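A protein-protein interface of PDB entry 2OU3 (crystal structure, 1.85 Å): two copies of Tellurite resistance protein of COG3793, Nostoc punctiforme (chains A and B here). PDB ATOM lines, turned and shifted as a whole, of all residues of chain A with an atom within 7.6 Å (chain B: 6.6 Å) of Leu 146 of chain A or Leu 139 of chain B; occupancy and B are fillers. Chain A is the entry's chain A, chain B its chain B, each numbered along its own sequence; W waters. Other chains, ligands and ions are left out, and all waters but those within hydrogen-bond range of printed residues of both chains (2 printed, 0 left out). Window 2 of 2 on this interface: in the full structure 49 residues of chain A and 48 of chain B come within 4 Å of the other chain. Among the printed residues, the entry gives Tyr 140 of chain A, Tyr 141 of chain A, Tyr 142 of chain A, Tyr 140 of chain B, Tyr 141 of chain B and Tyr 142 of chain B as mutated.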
ATOM      1  N   LEU A 139      19.342  32.808 -15.373  1.00  0.00           N
ATOM      2  CA  LEU A 139      18.969  33.352 -16.658  1.00  0.00           C
ATOM      3  C   LEU A 139      19.942  32.864 -17.771  1.00  0.00           C
ATOM      4  O   LEU A 139      19.498  32.387 -18.814  1.00  0.00           O
ATOM      5  CB  LEU A 139      18.934  34.853 -16.589  1.00  0.00           C
ATOM      6  CG  LEU A 139      18.562  35.551 -17.898  1.00  0.00           C
ATOM      7  CD1 LEU A 139      17.107  35.281 -18.272  1.00  0.00           C
ATOM      8  CD2 LEU A 139      18.837  37.028 -17.755  1.00  0.00           C
ATOM      9  N   TYR A 140      21.243  32.969 -17.513  1.00  0.00           N
ATOM     10  CA  TYR A 140      22.262  32.374 -18.376  1.00  0.00           C
ATOM     11  C   TYR A 140      21.915  30.905 -18.711  1.00  0.00           C
ATOM     12  O   TYR A 140      21.897  30.485 -19.893  1.00  0.00           O
ATOM     13  CB  TYR A 140      23.665  32.453 -17.749  1.00  0.00           C
ATOM     14  CG  TYR A 140      24.559  31.453 -18.415  1.00  0.00           C
ATOM     15  CD1 TYR A 140      25.000  31.675 -19.700  1.00  0.00           C
ATOM     16  CD2 TYR A 140      24.850  30.234 -17.826  1.00  0.00           C
ATOM     17  CE1 TYR A 140      25.734  30.758 -20.370  1.00  0.00           C
ATOM     18  CE2 TYR A 140      25.612  29.287 -18.511  1.00  0.00           C
ATOM     19  CZ  TYR A 140      26.031  29.564 -19.783  1.00  0.00           C
ATOM     20  OH  TYR A 140      26.765  28.672 -20.508  1.00  0.00           O
ATOM     21  N   TYR A 141      21.693  30.084 -17.693  1.00  0.00           N
ATOM     22  CA  TYR A 141      21.501  28.644 -17.974  1.00  0.00           C
ATOM     23  C   TYR A 141      20.282  28.438 -18.854  1.00  0.00           C
ATOM     24  O   TYR A 141      20.308  27.608 -19.751  1.00  0.00           O
ATOM     25  CB  TYR A 141      21.395  27.793 -16.711  1.00  0.00           C
ATOM     26  CG  TYR A 141      22.739  27.547 -16.058  1.00  0.00           C
ATOM     27  CD1 TYR A 141      23.691  26.728 -16.663  1.00  0.00           C
ATOM     28  CD2 TYR A 141      23.056  28.131 -14.830  1.00  0.00           C
ATOM     29  CE1 TYR A 141      24.929  26.508 -16.055  1.00  0.00           C
ATOM     30  CE2 TYR A 141      24.280  27.917 -14.223  1.00  0.00           C
ATOM     31  CZ  TYR A 141      25.207  27.117 -14.835  1.00  0.00           C
ATOM     32  OH  TYR A 141      26.402  26.914 -14.207  1.00  0.00           O
ATOM     33  N   TYR A 142      19.217  29.172 -18.555  1.00  0.00           N
ATOM     34  CA  TYR A 142      17.976  29.098 -19.335  1.00  0.00           C
ATOM     35  C   TYR A 142      18.160  29.606 -20.764  1.00  0.00           C
ATOM     36  O   TYR A 142      17.637  29.011 -21.710  1.00  0.00           O
ATOM     37  CB  TYR A 142      16.879  29.905 -18.664  1.00  0.00           C
ATOM     38  CG  TYR A 142      16.086  29.145 -17.629  1.00  0.00           C
ATOM     39  CD1 TYR A 142      16.571  28.985 -16.336  1.00  0.00           C
ATOM     40  CD2 TYR A 142      14.845  28.593 -17.938  1.00  0.00           C
ATOM     41  CE1 TYR A 142      15.855  28.291 -15.361  1.00  0.00           C
ATOM     42  CE2 TYR A 142      14.112  27.899 -16.968  1.00  0.00           C
ATOM     43  CZ  TYR A 142      14.636  27.754 -15.682  1.00  0.00           C
ATOM     44  OH  TYR A 142      13.942  27.082 -14.704  1.00  0.00           O
ATOM     45  N   GLU A 143      18.878  30.715 -20.919  1.00  0.00           N
ATOM     46  CA  GLU A 143      19.145  31.266 -22.250  1.00  0.00           C
ATOM     47  C   GLU A 143      19.981  30.294 -23.100  1.00  0.00           C
ATOM     48  O   GLU A 143      19.648  30.017 -24.258  1.00  0.00           O
ATOM     49  CB  GLU A 143      19.831  32.610 -22.140  1.00  0.00           C
ATOM     50  CG  GLU A 143      18.930  33.759 -21.754  1.00  0.00           C
ATOM     51  CD  GLU A 143      19.701  35.113 -21.556  1.00  0.00           C
ATOM     52  OE1 GLU A 143      20.951  35.142 -21.374  1.00  0.00           O
ATOM     53  OE2 GLU A 143      19.018  36.155 -21.487  1.00  0.00           O
ATOM     54  N   ALA A 144      21.014  29.728 -22.490  1.00  0.00           N
ATOM     55  CA  ALA A 144      21.906  28.777 -23.155  1.00  0.00           C
ATOM     56  C   ALA A 144      21.130  27.534 -23.573  1.00  0.00           C
ATOM     57  O   ALA A 144      21.236  27.072 -24.697  1.00  0.00           O
ATOM     58  CB  ALA A 144      23.071  28.426 -22.231  1.00  0.00           C
ATOM     59  N   ALA A 145      20.301  27.030 -22.662  1.00  0.00           N
ATOM     60  CA  ALA A 145      19.467  25.851 -22.927  1.00  0.00           C
ATOM     61  C   ALA A 145      18.425  26.062 -24.034  1.00  0.00           C
ATOM     62  O   ALA A 145      18.186  25.187 -24.865  1.00  0.00           O
ATOM     63  CB  ALA A 145      18.789  25.402 -21.622  1.00  0.00           C
ATOM     64  N   LEU A 146      17.797  27.220 -24.034  1.00  0.00           N
ATOM     65  CA  LEU A 146      16.778  27.549 -25.016  1.00  0.00           C
ATOM     66  C   LEU A 146      17.395  27.738 -26.404  1.00  0.00           C
ATOM     67  O   LEU A 146      16.792  27.382 -27.417  1.00  0.00           O
ATOM     68  CB  LEU A 146      16.012  28.803 -24.570  1.00  0.00           C
ATOM     69  CG  LEU A 146      14.756  29.163 -25.377  1.00  0.00           C
ATOM     70  CD1 LEU A 146      13.748  28.010 -25.469  1.00  0.00           C
ATOM     71  CD2 LEU A 146      14.106  30.435 -24.789  1.00  0.00           C
ATOM     72  N   ARG A 147      18.600  28.297 -26.455  1.00  0.00           N
ATOM     73  CA  ARG A 147      19.318  28.427 -27.723  1.00  0.00           C
ATOM     74  C   ARG A 147      19.639  27.065 -28.295  1.00  0.00           C
ATOM     75  O   ARG A 147      19.467  26.841 -29.487  1.00  0.00           O
ATOM     76  CB  ARG A 147      20.576  29.293 -27.564  1.00  0.00           C
ATOM     77  CG  ARG A 147      21.499  29.301 -28.770  1.00  0.00           C
ATOM     78  CD  ARG A 147      22.596  30.340 -28.691  1.00  0.00           C
ATOM     79  NE  ARG A 147      23.461  30.207 -29.858  1.00  0.00           N
ATOM     80  CZ  ARG A 147      24.378  29.257 -29.975  1.00  0.00           C
ATOM     81  NH1 ARG A 147      24.579  28.400 -28.984  1.00  0.00           N
ATOM     82  NH2 ARG A 147      25.105  29.165 -31.070  1.00  0.00           N
ATOM     83  N   GLN A 148      20.102  26.147 -27.457  1.00  0.00           N
ATOM     84  CA  GLN A 148      20.379  24.786 -27.886  1.00  0.00           C
ATOM     85  C   GLN A 148      19.128  24.091 -28.433  1.00  0.00           C
ATOM     86  O   GLN A 148      19.187  23.392 -29.462  1.00  0.00           O
ATOM     87  CB  GLN A 148      20.931  23.973 -26.725  1.00  0.00           C
ATOM     88  CG  GLN A 148      22.350  24.306 -26.350  1.00  0.00           C
ATOM     89  CD  GLN A 148      23.285  24.186 -27.531  1.00  0.00           C
ATOM     90  OE1 GLN A 148      23.267  23.173 -28.269  1.00  0.00           O
ATOM     91  NE2 GLN A 148      24.074  25.236 -27.760  1.00  0.00           N
ATOM     92  N   LYS A 149      18.010  24.285 -27.732  1.00  0.00           N
ATOM     93  CA  LYS A 149      16.709  23.778 -28.160  1.00  0.00           C
ATOM     94  C   LYS A 149      16.313  24.338 -29.524  1.00  0.00           C
ATOM     95  O   LYS A 149      15.893  23.576 -30.379  1.00  0.00           O
ATOM     96  CB  LYS A 149      15.634  24.117 -27.127  1.00  0.00           C
ATOM     97  CG  LYS A 149      14.246  23.621 -27.506  1.00  0.00           C
ATOM     98  CD  LYS A 149      13.421  23.315 -26.260  1.00  0.00           C
ATOM     99  CE  LYS A 149      12.053  22.739 -26.614  1.00  0.00           C
ATOM    100  NZ  LYS A 149      11.169  22.691 -25.407  1.00  0.00           N
ATOM    101  N   ARG A 150      16.471  25.649 -29.713  1.00  0.00           N
ATOM    102  CA  ARG A 150      16.232  26.308 -31.002  1.00  0.00           C
ATOM    103  C   ARG A 150      17.033  25.602 -32.098  1.00  0.00           C
ATOM    104  O   ARG A 150      16.478  25.140 -33.103  1.00  0.00           O
ATOM    105  CB  ARG A 150      16.630  27.797 -30.906  1.00  0.00           C
ATOM    106  CG  ARG A 150      16.164  28.719 -32.071  1.00  0.00           C
ATOM    107  CD  ARG A 150      17.183  29.857 -32.350  1.00  0.00           C
ATOM    108  NE  ARG A 150      16.624  31.216 -32.456  1.00  0.00           N
ATOM    109  CZ  ARG A 150      16.620  32.001 -33.539  1.00  0.00           C
ATOM    110  NH1 ARG A 150      17.123  31.612 -34.720  1.00  0.00           N
ATOM    111  NH2 ARG A 150      16.087  33.218 -33.440  1.00  0.00           N
ATOM    112  N   LEU A 151      18.336  25.531 -31.900  1.00  0.00           N
ATOM    113  CA  LEU A 151      19.234  25.034 -32.968  1.00  0.00           C
ATOM    114  C   LEU A 151      18.891  23.598 -33.327  1.00  0.00           C
ATOM    115  O   LEU A 151      18.898  23.245 -34.500  1.00  0.00           O
ATOM    116  CB  LEU A 151      20.693  25.130 -32.545  1.00  0.00           C
ATOM    117  CG  LEU A 151      21.155  26.590 -32.307  1.00  0.00           C
ATOM    118  CD1 LEU A 151      22.653  26.633 -32.015  1.00  0.00           C
ATOM    119  CD2 LEU A 151      20.767  27.465 -33.490  1.00  0.00           C
ATOM    120  N   ASN A 152      18.604  22.783 -32.318  1.00  0.00           N
ATOM    121  CA  ASN A 152      18.262  21.363 -32.554  1.00  0.00           C
ATOM    122  C   ASN A 152      16.911  21.169 -33.243  1.00  0.00           C
ATOM    123  O   ASN A 152      16.736  20.210 -34.001  1.00  0.00           O
ATOM    124  CB  ASN A 152      18.315  20.552 -31.251  1.00  0.00           C
ATOM    125  CG  ASN A 152      19.702  20.471 -30.671  1.00  0.00           C
ATOM    126  OD1 ASN A 152      20.704  20.525 -31.399  1.00  0.00           O
ATOM    127  ND2 ASN A 152      19.779  20.335 -29.344  1.00  0.00           N
ATOM    128  N   LEU A 153      15.977  22.080 -32.991  1.00  0.00           N
ATOM    129  CA  LEU A 153      14.685  22.088 -33.674  1.00  0.00           C
ATOM    130  C   LEU A 153      14.832  22.565 -35.141  1.00  0.00           C
ATOM    131  O   LEU A 153      14.236  21.980 -36.059  1.00  0.00           O
ATOM    132  CB  LEU A 153      13.702  22.962 -32.887  1.00  0.00           C
ATOM    133  CG  LEU A 153      12.227  22.971 -33.297  1.00  0.00           C
ATOM    134  CD1 LEU A 153      11.653  21.583 -33.213  1.00  0.00           C
ATOM    135  CD2 LEU A 153      11.423  23.959 -32.448  1.00  0.00           C
ATOM    136  N   LEU A 154      15.648  23.591 -35.379  1.00  0.00           N
ATOM    137  CA  LEU A 154      15.802  24.116 -36.743  1.00  0.00           C
ATOM    138  C   LEU A 154      16.573  23.160 -37.613  1.00  0.00           C
ATOM    139  O   LEU A 154      16.246  22.981 -38.798  1.00  0.00           O
ATOM    140  CB  LEU A 154      16.516  25.461 -36.713  1.00  0.00           C
ATOM    141  CG  LEU A 154      15.782  26.617 -36.017  1.00  0.00           C
ATOM    142  CD1 LEU A 154      16.512  27.910 -36.313  1.00  0.00           C
ATOM    143  CD2 LEU A 154      14.336  26.699 -36.447  1.00  0.00           C
ATOM    144  N   LEU B  99      10.407  30.005 -38.463  1.00  0.00           N
ATOM    145  CA  LEU B  99      10.593  30.655 -37.153  1.00  0.00           C
ATOM    146  C   LEU B  99      10.851  32.151 -37.313  1.00  0.00           C
ATOM    147  O   LEU B  99      10.276  32.986 -36.591  1.00  0.00           O
ATOM    148  CB  LEU B  99      11.735  29.983 -36.353  1.00  0.00           C
ATOM    149  CG  LEU B  99      12.007  30.551 -34.952  1.00  0.00           C
ATOM    150  CD1 LEU B  99      10.792  30.507 -34.002  1.00  0.00           C
ATOM    151  CD2 LEU B  99      13.233  29.925 -34.307  1.00  0.00           C
ATOM    152  N   TRP B 103       8.549  35.392 -35.903  1.00  0.00           N
ATOM    153  CA  TRP B 103       9.093  36.583 -35.237  1.00  0.00           C
ATOM    154  C   TRP B 103       8.738  37.858 -35.985  1.00  0.00           C
ATOM    155  O   TRP B 103       8.382  38.855 -35.392  1.00  0.00           O
ATOM    156  CB  TRP B 103      10.610  36.484 -35.113  1.00  0.00           C
ATOM    157  CG  TRP B 103      11.042  35.810 -33.879  1.00  0.00           C
ATOM    158  CD1 TRP B 103      11.414  34.502 -33.711  1.00  0.00           C
ATOM    159  CD2 TRP B 103      11.124  36.424 -32.596  1.00  0.00           C
ATOM    160  NE1 TRP B 103      11.720  34.284 -32.399  1.00  0.00           N
ATOM    161  CE2 TRP B 103      11.557  35.449 -31.699  1.00  0.00           C
ATOM    162  CE3 TRP B 103      10.890  37.718 -32.136  1.00  0.00           C
ATOM    163  CZ2 TRP B 103      11.753  35.726 -30.351  1.00  0.00           C
ATOM    164  CZ3 TRP B 103      11.084  37.987 -30.810  1.00  0.00           C
ATOM    165  CH2 TRP B 103      11.498  36.996 -29.941  1.00  0.00           C
ATOM    166  N   ASP B 134       3.619  23.871 -34.289  1.00  0.00           N
ATOM    167  CA  ASP B 134       3.252  24.200 -32.909  1.00  0.00           C
ATOM    168  C   ASP B 134       4.489  24.384 -32.020  1.00  0.00           C
ATOM    169  O   ASP B 134       4.508  25.238 -31.142  1.00  0.00           O
ATOM    170  CB  ASP B 134       2.274  23.160 -32.305  1.00  0.00           C
ATOM    171  CG  ASP B 134       0.892  23.232 -32.928  1.00  0.00           C
ATOM    172  OD1 ASP B 134       0.530  24.349 -33.357  1.00  0.00           O
ATOM    173  OD2 ASP B 134       0.155  22.201 -33.050  1.00  0.00           O
ATOM    174  N   GLN B 135       5.511  23.566 -32.247  1.00  0.00           N
ATOM    175  CA  GLN B 135       6.760  23.669 -31.493  1.00  0.00           C
ATOM    176  C   GLN B 135       7.523  24.936 -31.801  1.00  0.00           C
ATOM    177  O   GLN B 135       8.115  25.523 -30.907  1.00  0.00           O
ATOM    178  CB  GLN B 135       7.649  22.458 -31.750  1.00  0.00           C
ATOM    179  CG  GLN B 135       7.155  21.215 -30.990  1.00  0.00           C
ATOM    180  CD  GLN B 135       7.828  19.929 -31.389  1.00  0.00           C
ATOM    181  OE1 GLN B 135       8.961  19.928 -31.838  1.00  0.00           O
ATOM    182  NE2 GLN B 135       7.111  18.805 -31.223  1.00  0.00           N
ATOM    183  N   LEU B 136       7.516  25.352 -33.065  1.00  0.00           N
ATOM    184  CA  LEU B 136       8.199  26.578 -33.466  1.00  0.00           C
ATOM    185  C   LEU B 136       7.502  27.803 -32.856  1.00  0.00           C
ATOM    186  O   LEU B 136       8.152  28.722 -32.357  1.00  0.00           O
ATOM    187  CB  LEU B 136       8.317  26.667 -35.002  1.00  0.00           C
ATOM    188  CG  LEU B 136       9.265  25.637 -35.680  1.00  0.00           C
ATOM    189  CD1 LEU B 136       9.074  25.501 -37.243  1.00  0.00           C
ATOM    190  CD2 LEU B 136      10.730  25.907 -35.326  1.00  0.00           C
ATOM    191  N   GLU B 137       6.175  27.803 -32.880  1.00  0.00           N
ATOM    192  CA  GLU B 137       5.395  28.886 -32.261  1.00  0.00           C
ATOM    193  C   GLU B 137       5.631  28.946 -30.757  1.00  0.00           C
ATOM    194  O   GLU B 137       5.875  30.016 -30.198  1.00  0.00           O
ATOM    195  CB  GLU B 137       3.907  28.743 -32.590  1.00  0.00           C
ATOM    196  CG  GLU B 137       3.591  28.925 -34.050  1.00  0.00           C
ATOM    197  CD  GLU B 137       2.109  29.220 -34.332  1.00  0.00           C
ATOM    198  OE1 GLU B 137       1.247  29.117 -33.410  1.00  0.00           O
ATOM    199  OE2 GLU B 137       1.830  29.594 -35.493  1.00  0.00           O
ATOM    200  N   GLN B 138       5.621  27.795 -30.090  1.00  0.00           N
ATOM    201  CA  GLN B 138       5.943  27.728 -28.676  1.00  0.00           C
ATOM    202  C   GLN B 138       7.362  28.233 -28.390  1.00  0.00           C
ATOM    203  O   GLN B 138       7.588  28.900 -27.391  1.00  0.00           O
ATOM    204  CB  GLN B 138       5.789  26.296 -28.167  1.00  0.00           C
ATOM    205  CG  GLN B 138       6.077  26.106 -26.702  1.00  0.00           C
ATOM    206  CD  GLN B 138       5.955  24.646 -26.254  1.00  0.00           C
ATOM    207  OE1 GLN B 138       6.484  23.723 -26.901  1.00  0.00           O
ATOM    208  NE2 GLN B 138       5.258  24.436 -25.152  1.00  0.00           N
ATOM    209  N   LEU B 139       8.324  27.906 -29.251  1.00  0.00           N
ATOM    210  CA  LEU B 139       9.693  28.383 -29.083  1.00  0.00           C
ATOM    211  C   LEU B 139       9.762  29.914 -29.153  1.00  0.00           C
ATOM    212  O   LEU B 139      10.410  30.555 -28.331  1.00  0.00           O
ATOM    213  CB  LEU B 139      10.601  27.791 -30.161  1.00  0.00           C
ATOM    214  CG  LEU B 139      12.059  28.252 -30.185  1.00  0.00           C
ATOM    215  CD1 LEU B 139      12.766  27.837 -28.927  1.00  0.00           C
ATOM    216  CD2 LEU B 139      12.750  27.663 -31.434  1.00  0.00           C
ATOM    217  N   TYR B 140       9.089  30.478 -30.140  1.00  0.00           N
ATOM    218  CA  TYR B 140       8.906  31.922 -30.259  1.00  0.00           C
ATOM    219  C   TYR B 140       8.360  32.511 -28.936  1.00  0.00           C
ATOM    220  O   TYR B 140       8.922  33.461 -28.389  1.00  0.00           O
ATOM    221  CB  TYR B 140       8.004  32.285 -31.441  1.00  0.00           C
ATOM    222  CG  TYR B 140       7.431  33.633 -31.200  1.00  0.00           C
ATOM    223  CD1 TYR B 140       8.220  34.757 -31.319  1.00  0.00           C
ATOM    224  CD2 TYR B 140       6.119  33.782 -30.716  1.00  0.00           C
ATOM    225  CE1 TYR B 140       7.748  35.982 -31.013  1.00  0.00           C
ATOM    226  CE2 TYR B 140       5.630  35.025 -30.407  1.00  0.00           C
ATOM    227  CZ  TYR B 140       6.449  36.121 -30.548  1.00  0.00           C
ATOM    228  OH  TYR B 140       6.004  37.372 -30.221  1.00  0.00           O
ATOM    229  N   TYR B 141       7.275  31.956 -28.407  1.00  0.00           N
ATOM    230  CA  TYR B 141       6.682  32.532 -27.191  1.00  0.00           C
ATOM    231  C   TYR B 141       7.686  32.498 -26.029  1.00  0.00           C
ATOM    232  O   TYR B 141       7.848  33.473 -25.263  1.00  0.00           O
ATOM    233  CB  TYR B 141       5.390  31.797 -26.816  1.00  0.00           C
ATOM    234  CG  TYR B 141       4.194  32.230 -27.658  1.00  0.00           C
ATOM    235  CD1 TYR B 141       3.689  33.521 -27.564  1.00  0.00           C
ATOM    236  CD2 TYR B 141       3.599  31.352 -28.589  1.00  0.00           C
ATOM    237  CE1 TYR B 141       2.615  33.932 -28.351  1.00  0.00           C
ATOM    238  CE2 TYR B 141       2.521  31.753 -29.367  1.00  0.00           C
ATOM    239  CZ  TYR B 141       2.039  33.044 -29.248  1.00  0.00           C
ATOM    240  OH  TYR B 141       0.960  33.449 -30.010  1.00  0.00           O
ATOM    241  N   TYR B 142       8.374  31.372 -25.909  1.00  0.00           N
ATOM    242  CA  TYR B 142       9.355  31.208 -24.850  1.00  0.00           C
ATOM    243  C   TYR B 142      10.512  32.190 -24.970  1.00  0.00           C
ATOM    244  O   TYR B 142      10.922  32.788 -23.964  1.00  0.00           O
ATOM    245  CB  TYR B 142       9.884  29.782 -24.799  1.00  0.00           C
ATOM    246  CG  TYR B 142       9.044  28.872 -23.958  1.00  0.00           C
ATOM    247  CD1 TYR B 142       9.190  28.842 -22.578  1.00  0.00           C
ATOM    248  CD2 TYR B 142       8.114  28.028 -24.532  1.00  0.00           C
ATOM    249  CE1 TYR B 142       8.406  27.980 -21.786  1.00  0.00           C
ATOM    250  CE2 TYR B 142       7.322  27.170 -23.760  1.00  0.00           C
ATOM    251  CZ  TYR B 142       7.471  27.149 -22.394  1.00  0.00           C
ATOM    252  OH  TYR B 142       6.694  26.294 -21.647  1.00  0.00           O
ATOM    253  N   GLU B 143      11.050  32.298 -26.182  1.00  0.00           N
ATOM    254  CA  GLU B 143      12.165  33.176 -26.480  1.00  0.00           C
ATOM    255  C   GLU B 143      11.797  34.624 -26.199  1.00  0.00           C
ATOM    256  O   GLU B 143      12.590  35.351 -25.572  1.00  0.00           O
ATOM    257  CB  GLU B 143      12.580  33.056 -27.946  1.00  0.00           C
ATOM    258  CG  GLU B 143      13.284  31.763 -28.302  1.00  0.00           C
ATOM    259  CD  GLU B 143      13.738  31.680 -29.789  1.00  0.00           C
ATOM    260  OE1 GLU B 143      13.099  32.266 -30.712  1.00  0.00           O
ATOM    261  OE2 GLU B 143      14.733  30.956 -30.018  1.00  0.00           O
ATOM    262  N   ALA B 144      10.604  35.041 -26.652  1.00  0.00           N
ATOM    263  CA  ALA B 144      10.146  36.414 -26.448  1.00  0.00           C
ATOM    264  C   ALA B 144       9.942  36.709 -24.949  1.00  0.00           C
ATOM    265  O   ALA B 144      10.362  37.755 -24.437  1.00  0.00           O
ATOM    266  CB  ALA B 144       8.873  36.649 -27.208  1.00  0.00           C
ATOM    267  N   LEU B 146      11.454  35.073 -22.387  1.00  0.00           N
ATOM    268  CA  LEU B 146      12.778  35.031 -21.714  1.00  0.00           C
ATOM    269  C   LEU B 146      13.574  36.316 -21.947  1.00  0.00           C
ATOM    270  O   LEU B 146      14.263  36.835 -21.033  1.00  0.00           O
ATOM    271  CB  LEU B 146      13.582  33.820 -22.192  1.00  0.00           C
ATOM    272  CG  LEU B 146      14.890  33.507 -21.425  1.00  0.00           C
ATOM    273  CD1 LEU B 146      14.633  33.341 -19.946  1.00  0.00           C
ATOM    274  CD2 LEU B 146      15.564  32.253 -21.985  1.00  0.00           C
HETATM  275  O   HOH W   1      16.790  36.172 -22.593  1.00  0.00           O
HETATM  276  O   HOH W   2      16.374  30.406 -28.149  1.00  0.00           O
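The side-chain carboxylate of Glu 143 of chain B lies within salt-bridge range of the guanidinium group of Arg 150 of chain A, at 3.1 Å.
The indole nitrogen of Trp 103 of chain B sits at hydrogen-bond distance from the side-chain carboxylate of Glu 143 of chain B (3.0 Å).
Leu 139 of chain A touches Leu 146 of chain B (CD1 to CD1, 3.6 Å). Tyr 142 of chain A touches Leu 146 of chain B. Glu 143 of chain A touches Leu 146 of chain B. CD1 of Leu 146 of chain A touches CD1 of Leu 139 of chain B, 3.6 Å away. Glu 143 of chain B touches Leu 146 of chain A (CA to CD2, 3.8 Å). Leu 146 of chain A touches Leu 146 of chain B. Arg 150 of chain A touches Leu 99 of chain B. Gln 135 of chain B touches Leu 153 of chain A (OE1 to CD1, 3.4 Å). CD2 of Leu 153 of chain A touches CD2 of Leu 136 of chain B, 3.5 Å away. Leu 136 of chain B touches Leu 154 of chain A (CD2 to CD2, 3.9 Å).
Printed residues of chain B within 4 Å of Glu 143 of chain A: Leu 146. Of the printed residues of chain B, Leu 146 of chain A touches Leu 139 (3.6 Å), Glu 143 (3.8 Å) and Leu 146 (3.6 Å). Of the printed residues of chain B, Leu 154 of chain A touches Leu 136. Printed residues of chain A within 4 Å of Leu 136 of chain B: Leu 153 (3.5 Å) and Leu 154 (3.9 Å). Of the printed residues of chain A, Leu 139 of chain B touches Leu 146 (3.6 Å) and Arg 150 (3.6 Å). Of the printed residues of chain A, Glu 143 of chain B touches Leu 146 and Arg 150. Ala 144 of chain B touches none of the printed residues of chain A. The nearest printed residue of chain A that does not touch Leu 139 of chain B is Leu 153 of chain A (4.1 Å). The nearest printed residue of chain A that does not touch Leu 146 of chain B is Ala 144 of chain A (6.0 Å).
Of the 14 printed residues of chain B, 6 touch a printed residue of chain A. Hydrophobic or aromatic side chains of chain B within 4 Å of the printed part of chain A: Leu 99, Leu 136, Leu 139 and Leu 146. Along chain B the printed residues that touch a printed residue of chain A span positions 99 to 146. Hydrophobic or aromatic side chains of chain A within 4 Å of the printed part of chain B: Leu 139, Leu 146, Leu 153 and Leu 154. Among the printed residues, 12 pairs touch across the chains. Among the printed residues, Asp or Glu carboxylates within 4 Å of a Lys or Arg side-chain nitrogen of the other chain: Arg 150 of chain A with Glu 143 of chain B (3.1 Å).
Leu 139 of chain A touches Leu 146 of chain B, and with the chains exchanged Leu 146 of chain A touches Leu 139 of chain B. Tyr 142 of chain A touches Leu 146 of chain B, but with the chains exchanged Leu 146 of chain A does not touch Tyr 142 of chain B (4.004 Å). Glu 143 of chain A touches Leu 146 of chain B, and with the chains exchanged Leu 146 of chain A touches Glu 143 of chain B. Leu 146 of chain A touches its own counterpart, Leu 146 of chain B.
Water W1 lies within hydrogen-bond range of OE2 of Glu 143 of chain A (2.5 Å) and O of Leu 146 of chain B (3.0 Å). Water W2 bridges OE2 of Glu 143 of chain B (2.5 Å) and O of Leu 146 of chain A (3.1 Å).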
